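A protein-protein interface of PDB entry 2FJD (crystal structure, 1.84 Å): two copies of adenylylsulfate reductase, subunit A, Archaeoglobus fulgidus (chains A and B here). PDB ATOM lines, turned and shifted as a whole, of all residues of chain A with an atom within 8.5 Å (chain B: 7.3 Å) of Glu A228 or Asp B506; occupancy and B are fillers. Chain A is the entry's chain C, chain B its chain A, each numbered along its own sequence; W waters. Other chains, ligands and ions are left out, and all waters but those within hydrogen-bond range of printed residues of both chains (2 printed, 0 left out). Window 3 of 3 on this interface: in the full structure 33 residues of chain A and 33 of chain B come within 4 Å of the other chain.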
ATOM      1  N   VAL A   2      -4.239   7.615 -25.826  1.00  0.00           N
ATOM      2  CA  VAL A   2      -3.196   7.083 -24.957  1.00  0.00           C
ATOM      3  C   VAL A   2      -3.806   6.598 -23.647  1.00  0.00           C
ATOM      4  O   VAL A   2      -4.707   7.231 -23.104  1.00  0.00           O
ATOM      5  CB  VAL A   2      -2.140   8.158 -24.645  1.00  0.00           C
ATOM      6  CG1 VAL A   2      -1.016   7.553 -23.825  1.00  0.00           C
ATOM      7  CG2 VAL A   2      -1.596   8.744 -25.943  1.00  0.00           C
ATOM      8  N   TYR A   4      -2.846   5.003 -19.680  1.00  0.00           N
ATOM      9  CA  TYR A   4      -1.878   4.698 -18.627  1.00  0.00           C
ATOM     10  C   TYR A   4      -2.642   4.139 -17.428  1.00  0.00           C
ATOM     11  O   TYR A   4      -3.118   4.897 -16.587  1.00  0.00           O
ATOM     12  CB  TYR A   4      -1.131   5.951 -18.155  1.00  0.00           C
ATOM     13  CG  TYR A   4      -0.375   6.713 -19.212  1.00  0.00           C
ATOM     14  CD1 TYR A   4      -0.996   7.718 -19.952  1.00  0.00           C
ATOM     15  CD2 TYR A   4       0.976   6.460 -19.447  1.00  0.00           C
ATOM     16  CE1 TYR A   4      -0.289   8.458 -20.895  1.00  0.00           C
ATOM     17  CE2 TYR A   4       1.693   7.191 -20.393  1.00  0.00           C
ATOM     18  CZ  TYR A   4       1.052   8.189 -21.112  1.00  0.00           C
ATOM     19  OH  TYR A   4       1.751   8.917 -22.049  1.00  0.00           O
ATOM     20  N   PRO A 223      -9.057  11.651 -36.415  1.00  0.00           N
ATOM     21  CA  PRO A 223      -9.995  12.773 -36.289  1.00  0.00           C
ATOM     22  C   PRO A 223      -9.325  14.127 -36.519  1.00  0.00           C
ATOM     23  O   PRO A 223      -8.101  14.214 -36.639  1.00  0.00           O
ATOM     24  CB  PRO A 223     -10.503  12.650 -34.850  1.00  0.00           C
ATOM     25  CG  PRO A 223     -10.207  11.223 -34.475  1.00  0.00           C
ATOM     26  CD  PRO A 223      -8.871  10.993 -35.112  1.00  0.00           C
ATOM     27  N   SER A 225      -9.170  16.336 -34.386  1.00  0.00           N
ATOM     28  CA  SER A 225      -8.566  16.673 -33.105  1.00  0.00           C
ATOM     29  C   SER A 225      -7.871  15.386 -32.694  1.00  0.00           C
ATOM     30  O   SER A 225      -8.478  14.312 -32.705  1.00  0.00           O
ATOM     31  CB  SER A 225      -9.629  17.084 -32.090  1.00  0.00           C
ATOM     32  OG  SER A 225     -10.190  18.332 -32.459  1.00  0.00           O
ATOM     33  N   THR A 226      -6.596  15.490 -32.345  1.00  0.00           N
ATOM     34  CA  THR A 226      -5.808  14.316 -32.004  1.00  0.00           C
ATOM     35  C   THR A 226      -5.326  14.173 -30.562  1.00  0.00           C
ATOM     36  O   THR A 226      -4.650  13.195 -30.233  1.00  0.00           O
ATOM     37  CB  THR A 226      -4.595  14.238 -32.926  1.00  0.00           C
ATOM     38  OG1 THR A 226      -3.919  15.501 -32.922  1.00  0.00           O
ATOM     39  CG2 THR A 226      -5.036  13.922 -34.354  1.00  0.00           C
ATOM     40  N   GLY A 227      -5.657  15.140 -29.712  1.00  0.00           N
ATOM     41  CA  GLY A 227      -5.257  15.071 -28.315  1.00  0.00           C
ATOM     42  C   GLY A 227      -6.393  14.467 -27.509  1.00  0.00           C
ATOM     43  O   GLY A 227      -6.819  13.348 -27.797  1.00  0.00           O
ATOM     44  N   GLU A 228      -6.890  15.191 -26.508  1.00  0.00           N
ATOM     45  CA  GLU A 228      -8.005  14.687 -25.710  1.00  0.00           C
ATOM     46  C   GLU A 228      -9.222  14.581 -26.621  1.00  0.00           C
ATOM     47  O   GLU A 228      -9.987  13.624 -26.538  1.00  0.00           O
ATOM     48  CB  GLU A 228      -8.370  15.641 -24.567  1.00  0.00           C
ATOM     49  CG  GLU A 228      -7.317  15.869 -23.507  1.00  0.00           C
ATOM     50  CD  GLU A 228      -7.869  16.651 -22.320  1.00  0.00           C
ATOM     51  OE1 GLU A 228      -8.793  17.474 -22.520  1.00  0.00           O
ATOM     52  OE2 GLU A 228      -7.372  16.453 -21.192  1.00  0.00           O
ATOM     53  N   ALA A 229      -9.383  15.578 -27.492  1.00  0.00           N
ATOM     54  CA  ALA A 229     -10.524  15.641 -28.405  1.00  0.00           C
ATOM     55  C   ALA A 229     -10.596  14.542 -29.452  1.00  0.00           C
ATOM     56  O   ALA A 229     -11.474  14.554 -30.320  1.00  0.00           O
ATOM     57  CB  ALA A 229     -10.582  17.005 -29.072  1.00  0.00           C
ATOM     58  N   ALA A 230      -9.675  13.589 -29.388  1.00  0.00           N
ATOM     59  CA  ALA A 230      -9.730  12.467 -30.310  1.00  0.00           C
ATOM     60  C   ALA A 230     -10.976  11.709 -29.849  1.00  0.00           C
ATOM     61  O   ALA A 230     -11.534  10.893 -30.580  1.00  0.00           O
ATOM     62  CB  ALA A 230      -8.496  11.594 -30.161  1.00  0.00           C
ATOM     63  N   GLY A 231     -11.406  12.005 -28.623  1.00  0.00           N
ATOM     64  CA  GLY A 231     -12.582  11.358 -28.059  1.00  0.00           C
ATOM     65  C   GLY A 231     -13.884  11.976 -28.544  1.00  0.00           C
ATOM     66  O   GLY A 231     -14.961  11.397 -28.377  1.00  0.00           O
ATOM     67  N   ARG A 232     -13.794  13.159 -29.144  1.00  0.00           N
ATOM     68  CA  ARG A 232     -14.979  13.834 -29.649  1.00  0.00           C
ATOM     69  C   ARG A 232     -15.274  13.424 -31.090  1.00  0.00           C
ATOM     70  O   ARG A 232     -15.163  14.226 -32.017  1.00  0.00           O
ATOM     71  CB  ARG A 232     -14.820  15.355 -29.576  1.00  0.00           C
ATOM     72  CG  ARG A 232     -16.068  16.148 -30.006  1.00  0.00           C
ATOM     73  CD  ARG A 232     -17.023  16.443 -28.841  1.00  0.00           C
ATOM     74  NE  ARG A 232     -17.802  15.290 -28.389  1.00  0.00           N
ATOM     75  CZ  ARG A 232     -18.864  14.797 -29.019  1.00  0.00           C
ATOM     76  NH1 ARG A 232     -19.292  15.347 -30.149  1.00  0.00           N
ATOM     77  NH2 ARG A 232     -19.514  13.761 -28.508  1.00  0.00           N
ATOM     78  N   THR A 233     -15.629  12.161 -31.282  1.00  0.00           N
ATOM     79  CA  THR A 233     -15.991  11.697 -32.613  1.00  0.00           C
ATOM     80  C   THR A 233     -17.447  12.124 -32.771  1.00  0.00           C
ATOM     81  O   THR A 233     -18.187  12.156 -31.783  1.00  0.00           O
ATOM     82  CB  THR A 233     -15.902  10.162 -32.726  1.00  0.00           C
ATOM     83  OG1 THR A 233     -16.619   9.558 -31.641  1.00  0.00           O
ATOM     84  CG2 THR A 233     -14.460   9.711 -32.685  1.00  0.00           C
ATOM     85  N   ILE A 237     -18.480   7.030 -30.181  1.00  0.00           N
ATOM     86  CA  ILE A 237     -17.129   6.534 -29.986  1.00  0.00           C
ATOM     87  C   ILE A 237     -17.179   5.116 -29.414  1.00  0.00           C
ATOM     88  O   ILE A 237     -16.222   4.351 -29.534  1.00  0.00           O
ATOM     89  CB  ILE A 237     -16.336   7.455 -29.030  1.00  0.00           C
ATOM     90  CG1 ILE A 237     -14.855   7.070 -29.044  1.00  0.00           C
ATOM     91  CG2 ILE A 237     -16.906   7.361 -27.623  1.00  0.00           C
ATOM     92  CD1 ILE A 237     -13.967   8.039 -28.281  1.00  0.00           C
ATOM     93  N   VAL B   2       2.093  13.956 -24.993  1.00  0.00           N
ATOM     94  CA  VAL B   2       1.544  13.689 -23.634  1.00  0.00           C
ATOM     95  C   VAL B   2       2.680  13.356 -22.669  1.00  0.00           C
ATOM     96  O   VAL B   2       3.623  12.654 -23.029  1.00  0.00           O
ATOM     97  CB  VAL B   2       0.554  12.504 -23.661  1.00  0.00           C
ATOM     98  CG1 VAL B   2      -0.115  12.365 -22.304  1.00  0.00           C
ATOM     99  CG2 VAL B   2      -0.480  12.712 -24.761  1.00  0.00           C
ATOM    100  N   TYR B   3       2.593  13.869 -21.445  1.00  0.00           N
ATOM    101  CA  TYR B   3       3.626  13.613 -20.450  1.00  0.00           C
ATOM    102  C   TYR B   3       3.028  13.137 -19.134  1.00  0.00           C
ATOM    103  O   TYR B   3       2.087  13.737 -18.618  1.00  0.00           O
ATOM    104  CB  TYR B   3       4.457  14.880 -20.210  1.00  0.00           C
ATOM    105  CG  TYR B   3       5.568  14.708 -19.193  1.00  0.00           C
ATOM    106  CD1 TYR B   3       6.497  13.676 -19.315  1.00  0.00           C
ATOM    107  CD2 TYR B   3       5.697  15.585 -18.115  1.00  0.00           C
ATOM    108  CE1 TYR B   3       7.527  13.517 -18.394  1.00  0.00           C
ATOM    109  CE2 TYR B   3       6.731  15.436 -17.183  1.00  0.00           C
ATOM    110  CZ  TYR B   3       7.639  14.398 -17.331  1.00  0.00           C
ATOM    111  OH  TYR B   3       8.655  14.229 -16.417  1.00  0.00           O
ATOM    112  N   TYR B   4       3.580  12.052 -18.603  1.00  0.00           N
ATOM    113  CA  TYR B   4       3.126  11.485 -17.339  1.00  0.00           C
ATOM    114  C   TYR B   4       4.319  11.267 -16.415  1.00  0.00           C
ATOM    115  O   TYR B   4       4.948  10.211 -16.436  1.00  0.00           O
ATOM    116  CB  TYR B   4       2.401  10.157 -17.577  1.00  0.00           C
ATOM    117  CG  TYR B   4       0.932  10.317 -17.902  1.00  0.00           C
ATOM    118  CD1 TYR B   4       0.516  11.090 -18.986  1.00  0.00           C
ATOM    119  CD2 TYR B   4      -0.048   9.708 -17.114  1.00  0.00           C
ATOM    120  CE1 TYR B   4      -0.838  11.257 -19.278  1.00  0.00           C
ATOM    121  CE2 TYR B   4      -1.407   9.870 -17.399  1.00  0.00           C
ATOM    122  CZ  TYR B   4      -1.794  10.646 -18.484  1.00  0.00           C
ATOM    123  OH  TYR B   4      -3.131  10.814 -18.776  1.00  0.00           O
ATOM    124  N   PHE B 495      -0.010  24.304  -9.900  1.00  0.00           N
ATOM    125  CA  PHE B 495      -0.352  22.891  -9.826  1.00  0.00           C
ATOM    126  C   PHE B 495      -0.679  22.532  -8.378  1.00  0.00           C
ATOM    127  O   PHE B 495      -1.701  21.908  -8.097  1.00  0.00           O
ATOM    128  CB  PHE B 495       0.811  22.018 -10.308  1.00  0.00           C
ATOM    129  CG  PHE B 495       0.572  20.542 -10.128  1.00  0.00           C
ATOM    130  CD1 PHE B 495      -0.436  19.897 -10.840  1.00  0.00           C
ATOM    131  CD2 PHE B 495       1.334  19.804  -9.227  1.00  0.00           C
ATOM    132  CE1 PHE B 495      -0.683  18.536 -10.657  1.00  0.00           C
ATOM    133  CE2 PHE B 495       1.094  18.437  -9.035  1.00  0.00           C
ATOM    134  CZ  PHE B 495       0.083  17.803  -9.752  1.00  0.00           C
ATOM    135  N   SER B 502      -9.498  18.113  -8.733  1.00  0.00           N
ATOM    136  CA  SER B 502      -9.799  16.910  -9.505  1.00  0.00           C
ATOM    137  C   SER B 502      -8.984  15.711  -9.039  1.00  0.00           C
ATOM    138  O   SER B 502      -7.862  15.866  -8.564  1.00  0.00           O
ATOM    139  CB  SER B 502      -9.512  17.167 -10.987  1.00  0.00           C
ATOM    140  OG  SER B 502      -9.555  15.961 -11.733  1.00  0.00           O
ATOM    141  N   THR B 503      -9.548  14.515  -9.185  1.00  0.00           N
ATOM    142  CA  THR B 503      -8.856  13.296  -8.785  1.00  0.00           C
ATOM    143  C   THR B 503      -7.822  12.902  -9.835  1.00  0.00           C
ATOM    144  O   THR B 503      -7.041  11.970  -9.634  1.00  0.00           O
ATOM    145  CB  THR B 503      -9.839  12.120  -8.586  1.00  0.00           C
ATOM    146  OG1 THR B 503     -10.590  11.905  -9.791  1.00  0.00           O
ATOM    147  CG2 THR B 503     -10.796  12.415  -7.437  1.00  0.00           C
ATOM    148  N   ALA B 504      -7.824  13.618 -10.956  1.00  0.00           N
ATOM    149  CA  ALA B 504      -6.880  13.360 -12.039  1.00  0.00           C
ATOM    150  C   ALA B 504      -6.026  14.602 -12.244  1.00  0.00           C
ATOM    151  O   ALA B 504      -6.553  15.693 -12.466  1.00  0.00           O
ATOM    152  CB  ALA B 504      -7.630  13.023 -13.324  1.00  0.00           C
ATOM    153  N   ASP B 505      -4.709  14.436 -12.172  1.00  0.00           N
ATOM    154  CA  ASP B 505      -3.793  15.557 -12.338  1.00  0.00           C
ATOM    155  C   ASP B 505      -3.882  16.256 -13.685  1.00  0.00           C
ATOM    156  O   ASP B 505      -3.695  17.466 -13.756  1.00  0.00           O
ATOM    157  CB  ASP B 505      -2.342  15.116 -12.123  1.00  0.00           C
ATOM    158  CG  ASP B 505      -2.037  14.780 -10.678  1.00  0.00           C
ATOM    159  OD1 ASP B 505      -2.727  15.303  -9.779  1.00  0.00           O
ATOM    160  OD2 ASP B 505      -1.091  14.001 -10.447  1.00  0.00           O
ATOM    161  N   ASP B 506      -4.157  15.508 -14.752  1.00  0.00           N
ATOM    162  CA  ASP B 506      -4.228  16.126 -16.073  1.00  0.00           C
ATOM    163  C   ASP B 506      -5.603  16.551 -16.574  1.00  0.00           C
ATOM    164  O   ASP B 506      -5.745  16.933 -17.729  1.00  0.00           O
ATOM    165  CB  ASP B 506      -3.549  15.252 -17.133  1.00  0.00           C
ATOM    166  CG  ASP B 506      -3.974  13.805 -17.071  1.00  0.00           C
ATOM    167  OD1 ASP B 506      -5.173  13.535 -16.862  1.00  0.00           O
ATOM    168  OD2 ASP B 506      -3.098  12.935 -17.249  1.00  0.00           O
ATOM    169  N   VAL B 507      -6.619  16.472 -15.726  1.00  0.00           N
ATOM    170  CA  VAL B 507      -7.940  16.932 -16.126  1.00  0.00           C
ATOM    171  C   VAL B 507      -8.387  17.877 -15.025  1.00  0.00           C
ATOM    172  O   VAL B 507      -9.041  17.480 -14.059  1.00  0.00           O
ATOM    173  CB  VAL B 507      -8.950  15.784 -16.291  1.00  0.00           C
ATOM    174  CG1 VAL B 507     -10.297  16.348 -16.724  1.00  0.00           C
ATOM    175  CG2 VAL B 507      -8.446  14.799 -17.339  1.00  0.00           C
ATOM    176  N   ASN B 508      -8.007  19.138 -15.185  1.00  0.00           N
ATOM    177  CA  ASN B 508      -8.310  20.169 -14.209  1.00  0.00           C
ATOM    178  C   ASN B 508      -8.906  21.389 -14.899  1.00  0.00           C
ATOM    179  O   ASN B 508      -8.462  21.784 -15.980  1.00  0.00           O
ATOM    180  CB  ASN B 508      -7.022  20.543 -13.470  1.00  0.00           C
ATOM    181  CG  ASN B 508      -7.273  21.401 -12.251  1.00  0.00           C
ATOM    182  OD1 ASN B 508      -7.686  22.551 -12.361  1.00  0.00           O
ATOM    183  ND2 ASN B 508      -7.025  20.835 -11.074  1.00  0.00           N
ATOM    184  N   TYR B 511      -6.320  24.823 -14.858  1.00  0.00           N
ATOM    185  CA  TYR B 511      -5.006  24.865 -15.487  1.00  0.00           C
ATOM    186  C   TYR B 511      -4.850  23.891 -16.641  1.00  0.00           C
ATOM    187  O   TYR B 511      -5.619  22.941 -16.789  1.00  0.00           O
ATOM    188  CB  TYR B 511      -3.886  24.630 -14.456  1.00  0.00           C
ATOM    189  CG  TYR B 511      -3.843  23.257 -13.804  1.00  0.00           C
ATOM    190  CD1 TYR B 511      -3.617  22.100 -14.557  1.00  0.00           C
ATOM    191  CD2 TYR B 511      -3.977  23.123 -12.422  1.00  0.00           C
ATOM    192  CE1 TYR B 511      -3.526  20.846 -13.946  1.00  0.00           C
ATOM    193  CE2 TYR B 511      -3.886  21.879 -11.803  1.00  0.00           C
ATOM    194  CZ  TYR B 511      -3.661  20.746 -12.566  1.00  0.00           C
ATOM    195  OH  TYR B 511      -3.571  19.519 -11.950  1.00  0.00           O
ATOM    196  N   ILE B 512      -3.854  24.158 -17.475  1.00  0.00           N
ATOM    197  CA  ILE B 512      -3.536  23.296 -18.599  1.00  0.00           C
ATOM    198  C   ILE B 512      -2.077  22.912 -18.428  1.00  0.00           C
ATOM    199  O   ILE B 512      -1.275  23.714 -17.947  1.00  0.00           O
ATOM    200  CB  ILE B 512      -3.695  24.018 -19.960  1.00  0.00           C
ATOM    201  CG1 ILE B 512      -2.918  25.337 -19.953  1.00  0.00           C
ATOM    202  CG2 ILE B 512      -5.165  24.250 -20.257  1.00  0.00           C
ATOM    203  CD1 ILE B 512      -2.840  26.008 -21.312  1.00  0.00           C
ATOM    204  N   LEU B 513      -1.740  21.680 -18.792  1.00  0.00           N
ATOM    205  CA  LEU B 513      -0.365  21.217 -18.707  1.00  0.00           C
ATOM    206  C   LEU B 513       0.271  21.577 -20.040  1.00  0.00           C
ATOM    207  O   LEU B 513      -0.435  21.810 -21.024  1.00  0.00           O
ATOM    208  CB  LEU B 513      -0.334  19.709 -18.468  1.00  0.00           C
ATOM    209  CG  LEU B 513      -0.858  19.336 -17.077  1.00  0.00           C
ATOM    210  CD1 LEU B 513      -1.192  17.854 -17.016  1.00  0.00           C
ATOM    211  CD2 LEU B 513       0.189  19.720 -16.030  1.00  0.00           C
ATOM    212  N   TRP B 515       1.734  19.884 -22.436  1.00  0.00           N
ATOM    213  CA  TRP B 515       1.336  19.098 -23.598  1.00  0.00           C
ATOM    214  C   TRP B 515      -0.081  19.423 -24.064  1.00  0.00           C
ATOM    215  O   TRP B 515      -0.387  19.329 -25.252  1.00  0.00           O
ATOM    216  CB  TRP B 515       1.478  17.589 -23.331  1.00  0.00           C
ATOM    217  CG  TRP B 515       0.456  16.962 -22.402  1.00  0.00           C
ATOM    218  CD1 TRP B 515       0.620  16.677 -21.075  1.00  0.00           C
ATOM    219  CD2 TRP B 515      -0.849  16.482 -22.754  1.00  0.00           C
ATOM    220  NE1 TRP B 515      -0.497  16.043 -20.583  1.00  0.00           N
ATOM    221  CE2 TRP B 515      -1.415  15.912 -21.591  1.00  0.00           C
ATOM    222  CE3 TRP B 515      -1.596  16.480 -23.941  1.00  0.00           C
ATOM    223  CZ2 TRP B 515      -2.696  15.342 -21.578  1.00  0.00           C
ATOM    224  CZ3 TRP B 515      -2.875  15.912 -23.930  1.00  0.00           C
ATOM    225  CH2 TRP B 515      -3.409  15.351 -22.753  1.00  0.00           C
ATOM    226  N   GLN B 516      -0.939  19.822 -23.133  1.00  0.00           N
ATOM    227  CA  GLN B 516      -2.318  20.156 -23.468  1.00  0.00           C
ATOM    228  C   GLN B 516      -2.364  21.492 -24.205  1.00  0.00           C
ATOM    229  O   GLN B 516      -3.116  21.658 -25.164  1.00  0.00           O
ATOM    230  CB  GLN B 516      -3.158  20.205 -22.193  1.00  0.00           C
ATOM    231  CG  GLN B 516      -3.019  18.930 -21.368  1.00  0.00           C
ATOM    232  CD  GLN B 516      -3.865  18.932 -20.114  1.00  0.00           C
ATOM    233  OE1 GLN B 516      -3.893  19.910 -19.373  1.00  0.00           O
ATOM    234  NE2 GLN B 516      -4.552  17.827 -19.864  1.00  0.00           N
ATOM    235  N   VAL B 519      -0.952  20.854 -27.798  1.00  0.00           N
ATOM    236  CA  VAL B 519      -1.882  20.191 -28.711  1.00  0.00           C
ATOM    237  C   VAL B 519      -2.818  21.251 -29.283  1.00  0.00           C
ATOM    238  O   VAL B 519      -3.147  21.242 -30.472  1.00  0.00           O
ATOM    239  CB  VAL B 519      -2.738  19.128 -27.977  1.00  0.00           C
ATOM    240  CG1 VAL B 519      -3.933  18.732 -28.838  1.00  0.00           C
ATOM    241  CG2 VAL B 519      -1.893  17.904 -27.672  1.00  0.00           C
ATOM    242  N   ARG B 563       4.477  19.791 -13.221  1.00  0.00           N
ATOM    243  CA  ARG B 563       4.654  18.832 -12.134  1.00  0.00           C
ATOM    244  C   ARG B 563       6.099  18.526 -11.738  1.00  0.00           C
ATOM    245  O   ARG B 563       6.345  17.980 -10.664  1.00  0.00           O
ATOM    246  CB  ARG B 563       3.900  17.545 -12.484  1.00  0.00           C
ATOM    247  CG  ARG B 563       2.388  17.743 -12.504  1.00  0.00           C
ATOM    248  CD  ARG B 563       1.662  16.630 -13.245  1.00  0.00           C
ATOM    249  NE  ARG B 563       1.966  16.659 -14.673  1.00  0.00           N
ATOM    250  CZ  ARG B 563       1.436  15.833 -15.570  1.00  0.00           C
ATOM    251  NH1 ARG B 563       0.567  14.899 -15.192  1.00  0.00           N
ATOM    252  NH2 ARG B 563       1.775  15.942 -16.848  1.00  0.00           N
HETATM  253  O   HOH W   1      -3.629   9.825 -21.188  1.00  0.00           O
HETATM  254  O   HOH W   2      -5.750  14.673 -20.166  1.00  0.00           O
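The side-chain carboxylate (OE2) of Glu A228 sits at hydrogen-bond distance from the side-chain amide nitrogen (NE2) of Gln B516 (3.4 Å).
The side-chain hydroxyl (OH) of Tyr B4 is in hydrogen-bond range of the side-chain carboxylate (OD2) of Asp B506, at 2.6 Å. O of Asp B506 sits at hydrogen-bond distance from NE2 of Gln B516 (2.6 Å). N of Leu B513 is in hydrogen-bond range of OE1 of Gln B516, 2.8 Å away.
Among the printed residues, pairs that only touch across the chains: Tyr A4 with Val B2 (3.9 Å), Tyr A4 with Tyr B4 (3.3 Å), Gly A227 with Val B519 (3.9 Å) and Glu A228 with Asp B506 (3.9 Å).
Printed residues of chain B within 4 Å of Tyr A4: Val B2 and Tyr B4. Of the printed residues of chain B, Glu A228 touches Asp B506 and Gln B516. Ala A229 touches none of the printed residues of chain B. Arg A232 touches none of the printed residues of chain B. Of the printed residues of chain A, Val B2 touches Tyr A4 (3.9 Å). Asp B506 touches just one residue of chain A: Glu A228 (3.9 Å). Printed residues of chain A within 4 Å of Val B519: Gly A227. The nearest printed residue of chain B that does not touch Glu A228 is Trp B515 (4.01 Å).
Of the 13 printed residues of chain A, 3 touch a printed residue of chain B. Printed residues of chain A that touch a printed residue of chain B: Tyr A4, Gly A227 and Glu A228. Of the 18 printed residues of chain B, 5 touch a printed residue of chain A. Hydrophobic or aromatic side chains of chain B within 4 Å of the printed part of chain A: Val B2, Tyr B4 and Val B519. Among the printed residues, 5 pairs touch across the chains. Among the printed residues, no Asp or Glu carboxylate lies within 4 Å of a Lys or Arg side-chain nitrogen of the other chain.
Tyr A4 touches Val B2, but with the chains exchanged Val A2 does not touch Tyr B4 (5.8 Å). Tyr B4 touches its own counterpart, Tyr A4.
Water W2 lies within hydrogen-bond range of the side-chain carboxylate of Glu A228 (2.6 Å), the backbone carbonyl oxygen of Asp B506 (3.3 Å) and the side-chain amide nitrogen of Gln B516 (3.4 Å). Water W1 bridges OH of Tyr B4 (2.7 Å) and O of Val A2 (3.4 Å).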
